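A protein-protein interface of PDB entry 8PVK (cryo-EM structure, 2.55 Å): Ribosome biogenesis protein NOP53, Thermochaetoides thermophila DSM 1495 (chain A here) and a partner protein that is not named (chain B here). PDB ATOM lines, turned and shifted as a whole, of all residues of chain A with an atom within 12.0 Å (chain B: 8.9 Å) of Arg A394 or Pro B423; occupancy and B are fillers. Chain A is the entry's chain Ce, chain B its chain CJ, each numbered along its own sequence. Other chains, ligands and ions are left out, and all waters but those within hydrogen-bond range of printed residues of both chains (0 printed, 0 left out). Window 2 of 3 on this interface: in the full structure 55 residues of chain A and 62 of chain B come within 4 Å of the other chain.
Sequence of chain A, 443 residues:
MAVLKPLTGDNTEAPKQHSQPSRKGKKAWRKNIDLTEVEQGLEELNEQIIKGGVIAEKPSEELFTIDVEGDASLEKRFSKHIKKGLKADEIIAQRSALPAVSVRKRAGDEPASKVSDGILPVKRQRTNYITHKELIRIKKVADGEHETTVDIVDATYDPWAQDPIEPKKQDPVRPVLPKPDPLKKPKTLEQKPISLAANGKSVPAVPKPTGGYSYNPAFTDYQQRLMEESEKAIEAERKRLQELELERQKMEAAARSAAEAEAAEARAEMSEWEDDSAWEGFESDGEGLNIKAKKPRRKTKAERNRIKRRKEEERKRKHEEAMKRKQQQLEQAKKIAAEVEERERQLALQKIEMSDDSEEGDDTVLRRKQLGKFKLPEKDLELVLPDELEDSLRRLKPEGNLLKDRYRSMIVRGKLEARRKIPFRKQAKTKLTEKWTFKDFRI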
ATOM      1  N   TYR A 215     -15.794  15.047 -23.873  1.00  0.00           N
ATOM      2  CA  TYR A 215     -15.201  14.069 -22.966  1.00  0.00           C
ATOM      3  C   TYR A 215     -15.948  14.051 -21.641  1.00  0.00           C
ATOM      4  O   TYR A 215     -15.982  13.022 -20.957  1.00  0.00           O
ATOM      5  CB  TYR A 215     -13.723  14.378 -22.724  1.00  0.00           C
ATOM      6  CG  TYR A 215     -13.454  15.619 -21.896  1.00  0.00           C
ATOM      7  CD1 TYR A 215     -13.368  16.871 -22.480  1.00  0.00           C
ATOM      8  CD2 TYR A 215     -13.214  15.518 -20.527  1.00  0.00           C
ATOM      9  CE1 TYR A 215     -13.114  17.993 -21.716  1.00  0.00           C
ATOM     10  CE2 TYR A 215     -12.953  16.632 -19.762  1.00  0.00           C
ATOM     11  CZ  TYR A 215     -12.901  17.865 -20.361  1.00  0.00           C
ATOM     12  OH  TYR A 215     -12.637  18.977 -19.601  1.00  0.00           O
ATOM     13  N   ASN A 216     -16.539  15.184 -21.271  1.00  0.00           N
ATOM     14  CA  ASN A 216     -17.330  15.336 -20.053  1.00  0.00           C
ATOM     15  C   ASN A 216     -18.695  15.860 -20.479  1.00  0.00           C
ATOM     16  O   ASN A 216     -19.028  17.029 -20.255  1.00  0.00           O
ATOM     17  CB  ASN A 216     -16.638  16.285 -19.072  1.00  0.00           C
ATOM     18  CG  ASN A 216     -17.337  16.363 -17.732  1.00  0.00           C
ATOM     19  OD1 ASN A 216     -18.038  15.437 -17.326  1.00  0.00           O
ATOM     20  ND2 ASN A 216     -17.148  17.477 -17.034  1.00  0.00           N
ATOM     21  N   VAL A 384     -17.530   6.651 -25.230  1.00  0.00           N
ATOM     22  CA  VAL A 384     -16.982   6.145 -23.978  1.00  0.00           C
ATOM     23  C   VAL A 384     -18.083   5.402 -23.235  1.00  0.00           C
ATOM     24  O   VAL A 384     -19.126   5.979 -22.907  1.00  0.00           O
ATOM     25  CB  VAL A 384     -16.402   7.279 -23.123  1.00  0.00           C
ATOM     26  CG1 VAL A 384     -15.638   6.709 -21.941  1.00  0.00           C
ATOM     27  CG2 VAL A 384     -15.493   8.155 -23.962  1.00  0.00           C
ATOM     28  N   GLU A 388     -16.296   3.043 -18.450  1.00  0.00           N
ATOM     29  CA  GLU A 388     -15.003   3.616 -18.798  1.00  0.00           C
ATOM     30  C   GLU A 388     -14.965   5.135 -18.667  1.00  0.00           C
ATOM     31  O   GLU A 388     -13.997   5.757 -19.116  1.00  0.00           O
ATOM     32  CB  GLU A 388     -14.614   3.212 -20.223  1.00  0.00           C
ATOM     33  CG  GLU A 388     -14.903   1.761 -20.565  1.00  0.00           C
ATOM     34  CD  GLU A 388     -14.908   1.508 -22.060  1.00  0.00           C
ATOM     35  OE1 GLU A 388     -14.991   2.487 -22.830  1.00  0.00           O
ATOM     36  OE2 GLU A 388     -14.830   0.329 -22.464  1.00  0.00           O
ATOM     37  N   LEU A 389     -15.993   5.747 -18.081  1.00  0.00           N
ATOM     38  CA  LEU A 389     -15.985   7.191 -17.884  1.00  0.00           C
ATOM     39  C   LEU A 389     -14.945   7.599 -16.850  1.00  0.00           C
ATOM     40  O   LEU A 389     -14.740   6.916 -15.842  1.00  0.00           O
ATOM     41  CB  LEU A 389     -17.364   7.690 -17.452  1.00  0.00           C
ATOM     42  CG  LEU A 389     -18.249   8.313 -18.534  1.00  0.00           C
ATOM     43  CD1 LEU A 389     -18.697   7.285 -19.542  1.00  0.00           C
ATOM     44  CD2 LEU A 389     -19.448   9.004 -17.904  1.00  0.00           C
ATOM     45  N   GLU A 390     -14.288   8.725 -17.109  1.00  0.00           N
ATOM     46  CA  GLU A 390     -13.286   9.284 -16.221  1.00  0.00           C
ATOM     47  C   GLU A 390     -13.668  10.712 -15.859  1.00  0.00           C
ATOM     48  O   GLU A 390     -14.374  11.397 -16.602  1.00  0.00           O
ATOM     49  CB  GLU A 390     -11.894   9.254 -16.863  1.00  0.00           C
ATOM     50  CG  GLU A 390     -11.439   7.865 -17.278  1.00  0.00           C
ATOM     51  CD  GLU A 390     -10.981   7.021 -16.105  1.00  0.00           C
ATOM     52  OE1 GLU A 390     -10.685   7.594 -15.035  1.00  0.00           O
ATOM     53  OE2 GLU A 390     -10.915   5.784 -16.254  1.00  0.00           O
ATOM     54  N   ASP A 391     -13.192  11.155 -14.698  1.00  0.00           N
ATOM     55  CA  ASP A 391     -13.551  12.454 -14.149  1.00  0.00           C
ATOM     56  C   ASP A 391     -12.492  13.527 -14.382  1.00  0.00           C
ATOM     57  O   ASP A 391     -12.602  14.620 -13.818  1.00  0.00           O
ATOM     58  CB  ASP A 391     -13.869  12.317 -12.654  1.00  0.00           C
ATOM     59  CG  ASP A 391     -12.679  11.838 -11.819  1.00  0.00           C
ATOM     60  OD1 ASP A 391     -11.592  11.556 -12.369  1.00  0.00           O
ATOM     61  OD2 ASP A 391     -12.840  11.739 -10.585  1.00  0.00           O
ATOM     62  N   SER A 392     -11.476  13.246 -15.194  1.00  0.00           N
ATOM     63  CA  SER A 392     -10.395  14.192 -15.415  1.00  0.00           C
ATOM     64  C   SER A 392      -9.952  14.144 -16.870  1.00  0.00           C
ATOM     65  O   SER A 392     -10.147  13.149 -17.572  1.00  0.00           O
ATOM     66  CB  SER A 392      -9.202  13.908 -14.493  1.00  0.00           C
ATOM     67  OG  SER A 392      -8.710  12.595 -14.690  1.00  0.00           O
ATOM     68  N   LEU A 393      -9.349  15.250 -17.313  1.00  0.00           N
ATOM     69  CA  LEU A 393      -8.776  15.307 -18.653  1.00  0.00           C
ATOM     70  C   LEU A 393      -7.513  14.460 -18.756  1.00  0.00           C
ATOM     71  O   LEU A 393      -7.166  13.997 -19.848  1.00  0.00           O
ATOM     72  CB  LEU A 393      -8.475  16.762 -19.021  1.00  0.00           C
ATOM     73  CG  LEU A 393      -8.038  17.107 -20.445  1.00  0.00           C
ATOM     74  CD1 LEU A 393      -9.187  16.927 -21.415  1.00  0.00           C
ATOM     75  CD2 LEU A 393      -7.498  18.524 -20.513  1.00  0.00           C
ATOM     76  N   ARG A 394      -6.816  14.258 -17.634  1.00  0.00           N
ATOM     77  CA  ARG A 394      -5.574  13.491 -17.639  1.00  0.00           C
ATOM     78  C   ARG A 394      -5.817  12.025 -17.984  1.00  0.00           C
ATOM     79  O   ARG A 394      -5.059  11.430 -18.758  1.00  0.00           O
ATOM     80  CB  ARG A 394      -4.886  13.616 -16.281  1.00  0.00           C
ATOM     81  CG  ARG A 394      -3.647  12.759 -16.117  1.00  0.00           C
ATOM     82  CD  ARG A 394      -3.121  12.842 -14.696  1.00  0.00           C
ATOM     83  NE  ARG A 394      -4.156  12.532 -13.717  1.00  0.00           N
ATOM     84  CZ  ARG A 394      -4.502  11.306 -13.352  1.00  0.00           C
ATOM     85  NH1 ARG A 394      -3.909  10.239 -13.862  1.00  0.00           N
ATOM     86  NH2 ARG A 394      -5.467  11.146 -12.451  1.00  0.00           N
ATOM     87  N   ARG A 395      -6.875  11.431 -17.432  1.00  0.00           N
ATOM     88  CA  ARG A 395      -7.193  10.030 -17.666  1.00  0.00           C
ATOM     89  C   ARG A 395      -8.099   9.826 -18.875  1.00  0.00           C
ATOM     90  O   ARG A 395      -8.790   8.804 -18.952  1.00  0.00           O
ATOM     91  CB  ARG A 395      -7.839   9.420 -16.421  1.00  0.00           C
ATOM     92  CG  ARG A 395      -6.860   9.105 -15.305  1.00  0.00           C
ATOM     93  CD  ARG A 395      -7.477   8.166 -14.284  1.00  0.00           C
ATOM     94  NE  ARG A 395      -7.978   6.944 -14.902  1.00  0.00           N
ATOM     95  CZ  ARG A 395      -7.275   5.828 -15.036  1.00  0.00           C
ATOM     96  NH1 ARG A 395      -6.028   5.741 -14.604  1.00  0.00           N
ATOM     97  NH2 ARG A 395      -7.838   4.773 -15.617  1.00  0.00           N
ATOM     98  N   LEU A 396      -8.113  10.772 -19.808  1.00  0.00           N
ATOM     99  CA  LEU A 396      -8.943  10.653 -20.997  1.00  0.00           C
ATOM    100  C   LEU A 396      -8.417   9.541 -21.897  1.00  0.00           C
ATOM    101  O   LEU A 396      -7.210   9.309 -22.002  1.00  0.00           O
ATOM    102  CB  LEU A 396      -8.973  11.987 -21.754  1.00  0.00           C
ATOM    103  CG  LEU A 396      -9.909  12.264 -22.937  1.00  0.00           C
ATOM    104  CD1 LEU A 396     -10.165  13.748 -22.995  1.00  0.00           C
ATOM    105  CD2 LEU A 396      -9.351  11.818 -24.275  1.00  0.00           C
ATOM    106  N   LYS A 397      -9.345   8.850 -22.553  1.00  0.00           N
ATOM    107  CA  LYS A 397      -9.008   7.801 -23.508  1.00  0.00           C
ATOM    108  C   LYS A 397      -9.416   8.276 -24.894  1.00  0.00           C
ATOM    109  O   LYS A 397     -10.605   8.209 -25.244  1.00  0.00           O
ATOM    110  CB  LYS A 397      -9.725   6.496 -23.153  1.00  0.00           C
ATOM    111  CG  LYS A 397      -9.341   5.313 -24.022  1.00  0.00           C
ATOM    112  CD  LYS A 397      -7.893   4.929 -23.796  1.00  0.00           C
ATOM    113  CE  LYS A 397      -7.689   4.421 -22.379  1.00  0.00           C
ATOM    114  NZ  LYS A 397      -8.382   3.127 -22.144  1.00  0.00           N
ATOM    115  N   PRO A 398      -8.490   8.797 -25.702  1.00  0.00           N
ATOM    116  CA  PRO A 398      -8.863   9.273 -27.041  1.00  0.00           C
ATOM    117  C   PRO A 398      -9.308   8.124 -27.932  1.00  0.00           C
ATOM    118  O   PRO A 398      -8.705   7.049 -27.942  1.00  0.00           O
ATOM    119  CB  PRO A 398      -7.578   9.926 -27.565  1.00  0.00           C
ATOM    120  CG  PRO A 398      -6.485   9.435 -26.682  1.00  0.00           C
ATOM    121  CD  PRO A 398      -7.094   9.115 -25.360  1.00  0.00           C
ATOM    122  N   GLU A 399     -10.374   8.367 -28.687  1.00  0.00           N
ATOM    123  CA  GLU A 399     -11.032   7.331 -29.463  1.00  0.00           C
ATOM    124  C   GLU A 399     -10.983   7.665 -30.946  1.00  0.00           C
ATOM    125  O   GLU A 399     -10.901   8.830 -31.346  1.00  0.00           O
ATOM    126  CB  GLU A 399     -12.486   7.146 -29.013  1.00  0.00           C
ATOM    127  CG  GLU A 399     -12.618   6.531 -27.632  1.00  0.00           C
ATOM    128  CD  GLU A 399     -14.058   6.371 -27.200  1.00  0.00           C
ATOM    129  OE1 GLU A 399     -14.951   6.886 -27.904  1.00  0.00           O
ATOM    130  OE2 GLU A 399     -14.298   5.727 -26.158  1.00  0.00           O
ATOM    131  N   TYR B 212      -4.873  14.948 -29.598  1.00  0.00           N
ATOM    132  CA  TYR B 212      -4.165  15.020 -28.329  1.00  0.00           C
ATOM    133  C   TYR B 212      -2.742  14.503 -28.501  1.00  0.00           C
ATOM    134  O   TYR B 212      -2.475  13.609 -29.307  1.00  0.00           O
ATOM    135  CB  TYR B 212      -4.889  14.205 -27.257  1.00  0.00           C
ATOM    136  CG  TYR B 212      -6.239  14.754 -26.856  1.00  0.00           C
ATOM    137  CD1 TYR B 212      -6.343  15.935 -26.135  1.00  0.00           C
ATOM    138  CD2 TYR B 212      -7.408  14.082 -27.186  1.00  0.00           C
ATOM    139  CE1 TYR B 212      -7.574  16.438 -25.761  1.00  0.00           C
ATOM    140  CE2 TYR B 212      -8.644  14.576 -26.816  1.00  0.00           C
ATOM    141  CZ  TYR B 212      -8.720  15.755 -26.105  1.00  0.00           C
ATOM    142  OH  TYR B 212      -9.948  16.249 -25.736  1.00  0.00           O
ATOM    143  N   PHE B 214      -0.303  12.349 -28.068  1.00  0.00           N
ATOM    144  CA  PHE B 214      -0.007  10.975 -27.685  1.00  0.00           C
ATOM    145  C   PHE B 214       0.649  10.292 -28.879  1.00  0.00           C
ATOM    146  O   PHE B 214       1.056  10.944 -29.846  1.00  0.00           O
ATOM    147  CB  PHE B 214      -1.274  10.237 -27.232  1.00  0.00           C
ATOM    148  CG  PHE B 214      -1.834  10.726 -25.929  1.00  0.00           C
ATOM    149  CD1 PHE B 214      -1.112  10.592 -24.755  1.00  0.00           C
ATOM    150  CD2 PHE B 214      -3.090  11.307 -25.874  1.00  0.00           C
ATOM    151  CE1 PHE B 214      -1.627  11.036 -23.552  1.00  0.00           C
ATOM    152  CE2 PHE B 214      -3.612  11.754 -24.675  1.00  0.00           C
ATOM    153  CZ  PHE B 214      -2.879  11.618 -23.513  1.00  0.00           C
ATOM    154  N   ARG B 376       2.948  20.028 -15.070  1.00  0.00           N
ATOM    155  CA  ARG B 376       3.440  19.233 -16.189  1.00  0.00           C
ATOM    156  C   ARG B 376       2.418  18.227 -16.706  1.00  0.00           C
ATOM    157  O   ARG B 376       2.546  17.770 -17.845  1.00  0.00           O
ATOM    158  CB  ARG B 376       4.735  18.525 -15.785  1.00  0.00           C
ATOM    159  CG  ARG B 376       4.563  17.119 -15.243  1.00  0.00           C
ATOM    160  CD  ARG B 376       5.909  16.498 -14.915  1.00  0.00           C
ATOM    161  NE  ARG B 376       6.560  17.170 -13.798  1.00  0.00           N
ATOM    162  CZ  ARG B 376       6.736  16.631 -12.600  1.00  0.00           C
ATOM    163  NH1 ARG B 376       6.315  15.407 -12.324  1.00  0.00           N
ATOM    164  NH2 ARG B 376       7.349  17.336 -11.654  1.00  0.00           N
ATOM    165  N   GLU B 377       1.391  17.903 -15.926  1.00  0.00           N
ATOM    166  CA  GLU B 377       0.388  16.929 -16.337  1.00  0.00           C
ATOM    167  C   GLU B 377      -0.731  17.543 -17.167  1.00  0.00           C
ATOM    168  O   GLU B 377      -1.671  16.831 -17.539  1.00  0.00           O
ATOM    169  CB  GLU B 377      -0.203  16.231 -15.108  1.00  0.00           C
ATOM    170  CG  GLU B 377      -1.160  17.089 -14.299  1.00  0.00           C
ATOM    171  CD  GLU B 377      -0.452  17.985 -13.305  1.00  0.00           C
ATOM    172  OE1 GLU B 377       0.790  17.910 -13.206  1.00  0.00           O
ATOM    173  OE2 GLU B 377      -1.141  18.760 -12.611  1.00  0.00           O
ATOM    174  N   THR B 378      -0.655  18.823 -17.463  1.00  0.00           N
ATOM    175  CA  THR B 378      -1.645  19.589 -18.196  1.00  0.00           C
ATOM    176  C   THR B 378      -1.187  19.819 -19.634  1.00  0.00           C
ATOM    177  O   THR B 378       0.015  19.933 -19.896  1.00  0.00           O
ATOM    178  CB  THR B 378      -1.880  20.933 -17.504  1.00  0.00           C
ATOM    179  OG1 THR B 378      -0.692  21.726 -17.585  1.00  0.00           O
ATOM    180  CG2 THR B 378      -2.213  20.700 -16.041  1.00  0.00           C
ATOM    181  N   PRO B 379      -2.120  19.889 -20.600  1.00  0.00           N
ATOM    182  CA  PRO B 379      -1.712  20.031 -22.006  1.00  0.00           C
ATOM    183  C   PRO B 379      -1.163  21.413 -22.343  1.00  0.00           C
ATOM    184  O   PRO B 379      -1.909  22.382 -22.560  1.00  0.00           O
ATOM    185  CB  PRO B 379      -3.005  19.724 -22.770  1.00  0.00           C
ATOM    186  CG  PRO B 379      -4.097  20.039 -21.814  1.00  0.00           C
ATOM    187  CD  PRO B 379      -3.570  19.663 -20.467  1.00  0.00           C
ATOM    188  N   ILE B 420      -3.766  22.584 -12.739  1.00  0.00           N
ATOM    189  CA  ILE B 420      -3.322  21.263 -12.308  1.00  0.00           C
ATOM    190  C   ILE B 420      -4.382  20.230 -12.662  1.00  0.00           C
ATOM    191  O   ILE B 420      -5.563  20.543 -12.828  1.00  0.00           O
ATOM    192  CB  ILE B 420      -3.005  21.183 -10.795  1.00  0.00           C
ATOM    193  CG1 ILE B 420      -4.240  21.465  -9.946  1.00  0.00           C
ATOM    194  CG2 ILE B 420      -1.892  22.136 -10.412  1.00  0.00           C
ATOM    195  CD1 ILE B 420      -4.008  21.162  -8.487  1.00  0.00           C
ATOM    196  N   ASP B 421      -3.936  18.980 -12.786  1.00  0.00           N
ATOM    197  CA  ASP B 421      -4.816  17.852 -13.077  1.00  0.00           C
ATOM    198  C   ASP B 421      -4.400  16.623 -12.276  1.00  0.00           C
ATOM    199  O   ASP B 421      -4.391  15.501 -12.793  1.00  0.00           O
ATOM    200  CB  ASP B 421      -4.834  17.541 -14.572  1.00  0.00           C
ATOM    201  CG  ASP B 421      -6.188  17.058 -15.051  1.00  0.00           C
ATOM    202  OD1 ASP B 421      -7.118  16.975 -14.224  1.00  0.00           O
ATOM    203  OD2 ASP B 421      -6.319  16.760 -16.257  1.00  0.00           O
ATOM    204  N   ARG B 422      -4.041  16.814 -11.002  1.00  0.00           N
ATOM    205  CA  ARG B 422      -3.661  15.692 -10.153  1.00  0.00           C
ATOM    206  C   ARG B 422      -4.699  15.460  -9.059  1.00  0.00           C
ATOM    207  O   ARG B 422      -5.345  16.406  -8.598  1.00  0.00           O
ATOM    208  CB  ARG B 422      -2.293  15.916  -9.496  1.00  0.00           C
ATOM    209  CG  ARG B 422      -1.159  16.147 -10.468  1.00  0.00           C
ATOM    210  CD  ARG B 422       0.178  16.232  -9.751  1.00  0.00           C
ATOM    211  NE  ARG B 422       0.829  14.932  -9.650  1.00  0.00           N
ATOM    212  CZ  ARG B 422       1.644  14.430 -10.568  1.00  0.00           C
ATOM    213  NH1 ARG B 422       1.928  15.093 -11.676  1.00  0.00           N
ATOM    214  NH2 ARG B 422       2.187  13.233 -10.368  1.00  0.00           N
ATOM    215  N   PRO B 423      -4.887  14.206  -8.616  1.00  0.00           N
ATOM    216  CA  PRO B 423      -5.796  13.934  -7.499  1.00  0.00           C
ATOM    217  C   PRO B 423      -5.197  14.332  -6.153  1.00  0.00           C
ATOM    218  O   PRO B 423      -5.609  15.346  -5.591  1.00  0.00           O
ATOM    219  CB  PRO B 423      -6.002  12.420  -7.576  1.00  0.00           C
ATOM    220  CG  PRO B 423      -4.758  11.912  -8.211  1.00  0.00           C
ATOM    221  CD  PRO B 423      -4.352  12.964  -9.202  1.00  0.00           C
ATOM    222  N   ARG B 449      -1.463  23.573  -0.808  1.00  0.00           N
ATOM    223  CA  ARG B 449      -1.863  24.628  -1.727  1.00  0.00           C
ATOM    224  C   ARG B 449      -1.317  25.961  -1.236  1.00  0.00           C
ATOM    225  O   ARG B 449      -1.493  26.318  -0.066  1.00  0.00           O
ATOM    226  CB  ARG B 449      -3.386  24.696  -1.860  1.00  0.00           C
ATOM    227  CG  ARG B 449      -3.979  23.595  -2.723  1.00  0.00           C
ATOM    228  CD  ARG B 449      -5.412  23.292  -2.321  1.00  0.00           C
ATOM    229  NE  ARG B 449      -6.328  24.341  -2.753  1.00  0.00           N
ATOM    230  CZ  ARG B 449      -7.471  24.123  -3.389  1.00  0.00           C
ATOM    231  NH1 ARG B 449      -7.875  22.898  -3.682  1.00  0.00           N
ATOM    232  NH2 ARG B 449      -8.226  25.160  -3.740  1.00  0.00           N
ATOM    233  N   GLN B 457      -8.658  23.120 -12.661  1.00  0.00           N
ATOM    234  CA  GLN B 457      -8.526  22.099 -13.685  1.00  0.00           C
ATOM    235  C   GLN B 457      -8.588  22.743 -15.071  1.00  0.00           C
ATOM    236  O   GLN B 457      -9.071  23.869 -15.213  1.00  0.00           O
ATOM    237  CB  GLN B 457      -9.634  21.061 -13.505  1.00  0.00           C
ATOM    238  CG  GLN B 457      -9.693  20.469 -12.105  1.00  0.00           C
ATOM    239  CD  GLN B 457     -10.427  19.145 -12.060  1.00  0.00           C
ATOM    240  OE1 GLN B 457     -10.359  18.355 -13.000  1.00  0.00           O
ATOM    241  NE2 GLN B 457     -11.134  18.897 -10.965  1.00  0.00           N
ATOM    242  N   PRO B 458      -8.077  22.064 -16.110  1.00  0.00           N
ATOM    243  CA  PRO B 458      -8.024  22.691 -17.445  1.00  0.00           C
ATOM    244  C   PRO B 458      -9.372  23.050 -18.062  1.00  0.00           C
ATOM    245  O   PRO B 458      -9.402  23.910 -18.948  1.00  0.00           O
ATOM    246  CB  PRO B 458      -7.296  21.640 -18.293  1.00  0.00           C
ATOM    247  CG  PRO B 458      -6.461  20.906 -17.331  1.00  0.00           C
ATOM    248  CD  PRO B 458      -7.249  20.843 -16.061  1.00  0.00           C
ATOM    249  N   ALA B 477     -12.417  23.566  -8.775  1.00  0.00           N
ATOM    250  CA  ALA B 477     -11.435  23.279  -7.745  1.00  0.00           C
ATOM    251  C   ALA B 477     -10.886  21.861  -7.906  1.00  0.00           C
ATOM    252  O   ALA B 477     -11.576  20.977  -8.420  1.00  0.00           O
ATOM    253  CB  ALA B 477     -12.066  23.452  -6.364  1.00  0.00           C
ATOM    254  N   PRO B 478      -9.631  21.632  -7.510  1.00  0.00           N
ATOM    255  CA  PRO B 478      -9.027  20.302  -7.683  1.00  0.00           C
ATOM    256  C   PRO B 478      -9.736  19.241  -6.855  1.00  0.00           C
ATOM    257  O   PRO B 478     -10.057  19.451  -5.682  1.00  0.00           O
ATOM    258  CB  PRO B 478      -7.583  20.507  -7.213  1.00  0.00           C
ATOM    259  CG  PRO B 478      -7.346  21.965  -7.330  1.00  0.00           C
ATOM    260  CD  PRO B 478      -8.646  22.620  -7.036  1.00  0.00           C
ATOM    261  N   GLY B 479      -9.978  18.089  -7.479  1.00  0.00           N
ATOM    262  CA  GLY B 479     -10.672  16.994  -6.842  1.00  0.00           C
ATOM    263  C   GLY B 479     -12.181  17.074  -6.901  1.00  0.00           C
ATOM    264  O   GLY B 479     -12.851  16.122  -6.479  1.00  0.00           O
ATOM    265  N   ALA B 480     -12.737  18.169  -7.409  1.00  0.00           N
ATOM    266  CA  ALA B 480     -14.179  18.327  -7.477  1.00  0.00           C
ATOM    267  C   ALA B 480     -14.723  17.763  -8.785  1.00  0.00           C
ATOM    268  O   ALA B 480     -13.991  17.538  -9.753  1.00  0.00           O
ATOM    269  CB  ALA B 480     -14.566  19.801  -7.342  1.00  0.00           C
ATOM    270  N   LEU B 482     -16.402  18.135 -12.158  1.00  0.00           N
ATOM    271  CA  LEU B 482     -16.450  19.243 -13.094  1.00  0.00           C
ATOM    272  C   LEU B 482     -17.861  19.422 -13.655  1.00  0.00           C
ATOM    273  O   LEU B 482     -18.623  18.457 -13.762  1.00  0.00           O
ATOM    274  CB  LEU B 482     -15.468  19.014 -14.239  1.00  0.00           C
ATOM    275  CG  LEU B 482     -13.984  18.986 -13.879  1.00  0.00           C
ATOM    276  CD1 LEU B 482     -13.250  17.977 -14.744  1.00  0.00           C
ATOM    277  CD2 LEU B 482     -13.375  20.369 -14.030  1.00  0.00           C
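The side-chain carboxylate of Asp B421 sits at hydrogen-bond distance from the backbone NH of Arg A394 (2.9 Å).
OG of Ser A392 sits at hydrogen-bond distance from N of Arg A395. The backbone NH (N) of Asp B421 lies within hydrogen-bond range of the side-chain carboxylate (OE2) of Glu B377 (2.8 Å).
Among the printed residues, pairs that only touch across the chains: Asn A216 with Leu B482 (3.6 Å), Asp A391 with Leu B482 (3.5 Å), Ser A392 with Asp B421 (3.7 Å), Leu A393 with Pro B379 (3.9 Å), Leu A393 with Asp B421 (3.5 Å), Leu A393 with Pro B458 (3.8 Å), Arg A394 with Pro B423 (3.9 Å), Leu A396 with Tyr B212 (3.7 Å) and Pro A398 with Phe B214 (3.96 Å).
Of chain B, only Asp B421 (2.9 Å) and Pro B423 (3.9 Å) come within 4 Å of Arg A394. Pro B423 touches just one residue of chain A: Arg A394 (3.9 Å). No residue of chain A comes within 4 Å of Glu B377. Of chain A, only Ser A392 (3.7 Å), Leu A393 (3.5 Å) and Arg A394 (2.9 Å) come within 4 Å of Asp B421. No residue of chain A comes within 4 Å of Arg B422. No residue of chain A comes within 4 Å of Gly B479. Printed residues of chain B within 4 Å of Ser A392: Asp B421. Of the printed residues of chain A, Tyr B212 touches Leu A396 (3.7 Å). Of the printed residues of chain B, Pro A398 touches Phe B214. Gln B457 touches none of the printed residues of chain A. The nearest residue of chain A that does not touch Pro B423 is Ser A392 (7.0 Å). The nearest printed residue of chain B that does not touch Leu A396 is Phe B214 (5.1 Å).
Printed residues of chain B that touch a printed residue of chain A: Tyr B212, Phe B214, Pro B379, Asp B421, Pro B423, Pro B458 and Leu B482. Printed residues of chain A that touch a printed residue of chain B: Asn A216, Asp A391, Ser A392, Leu A393, Arg A394, Leu A396 and Pro A398. Hydrophobic or aromatic side chains of chain A within 4 Å of the printed part of chain B: Leu A393, Leu A396 and Pro A398.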
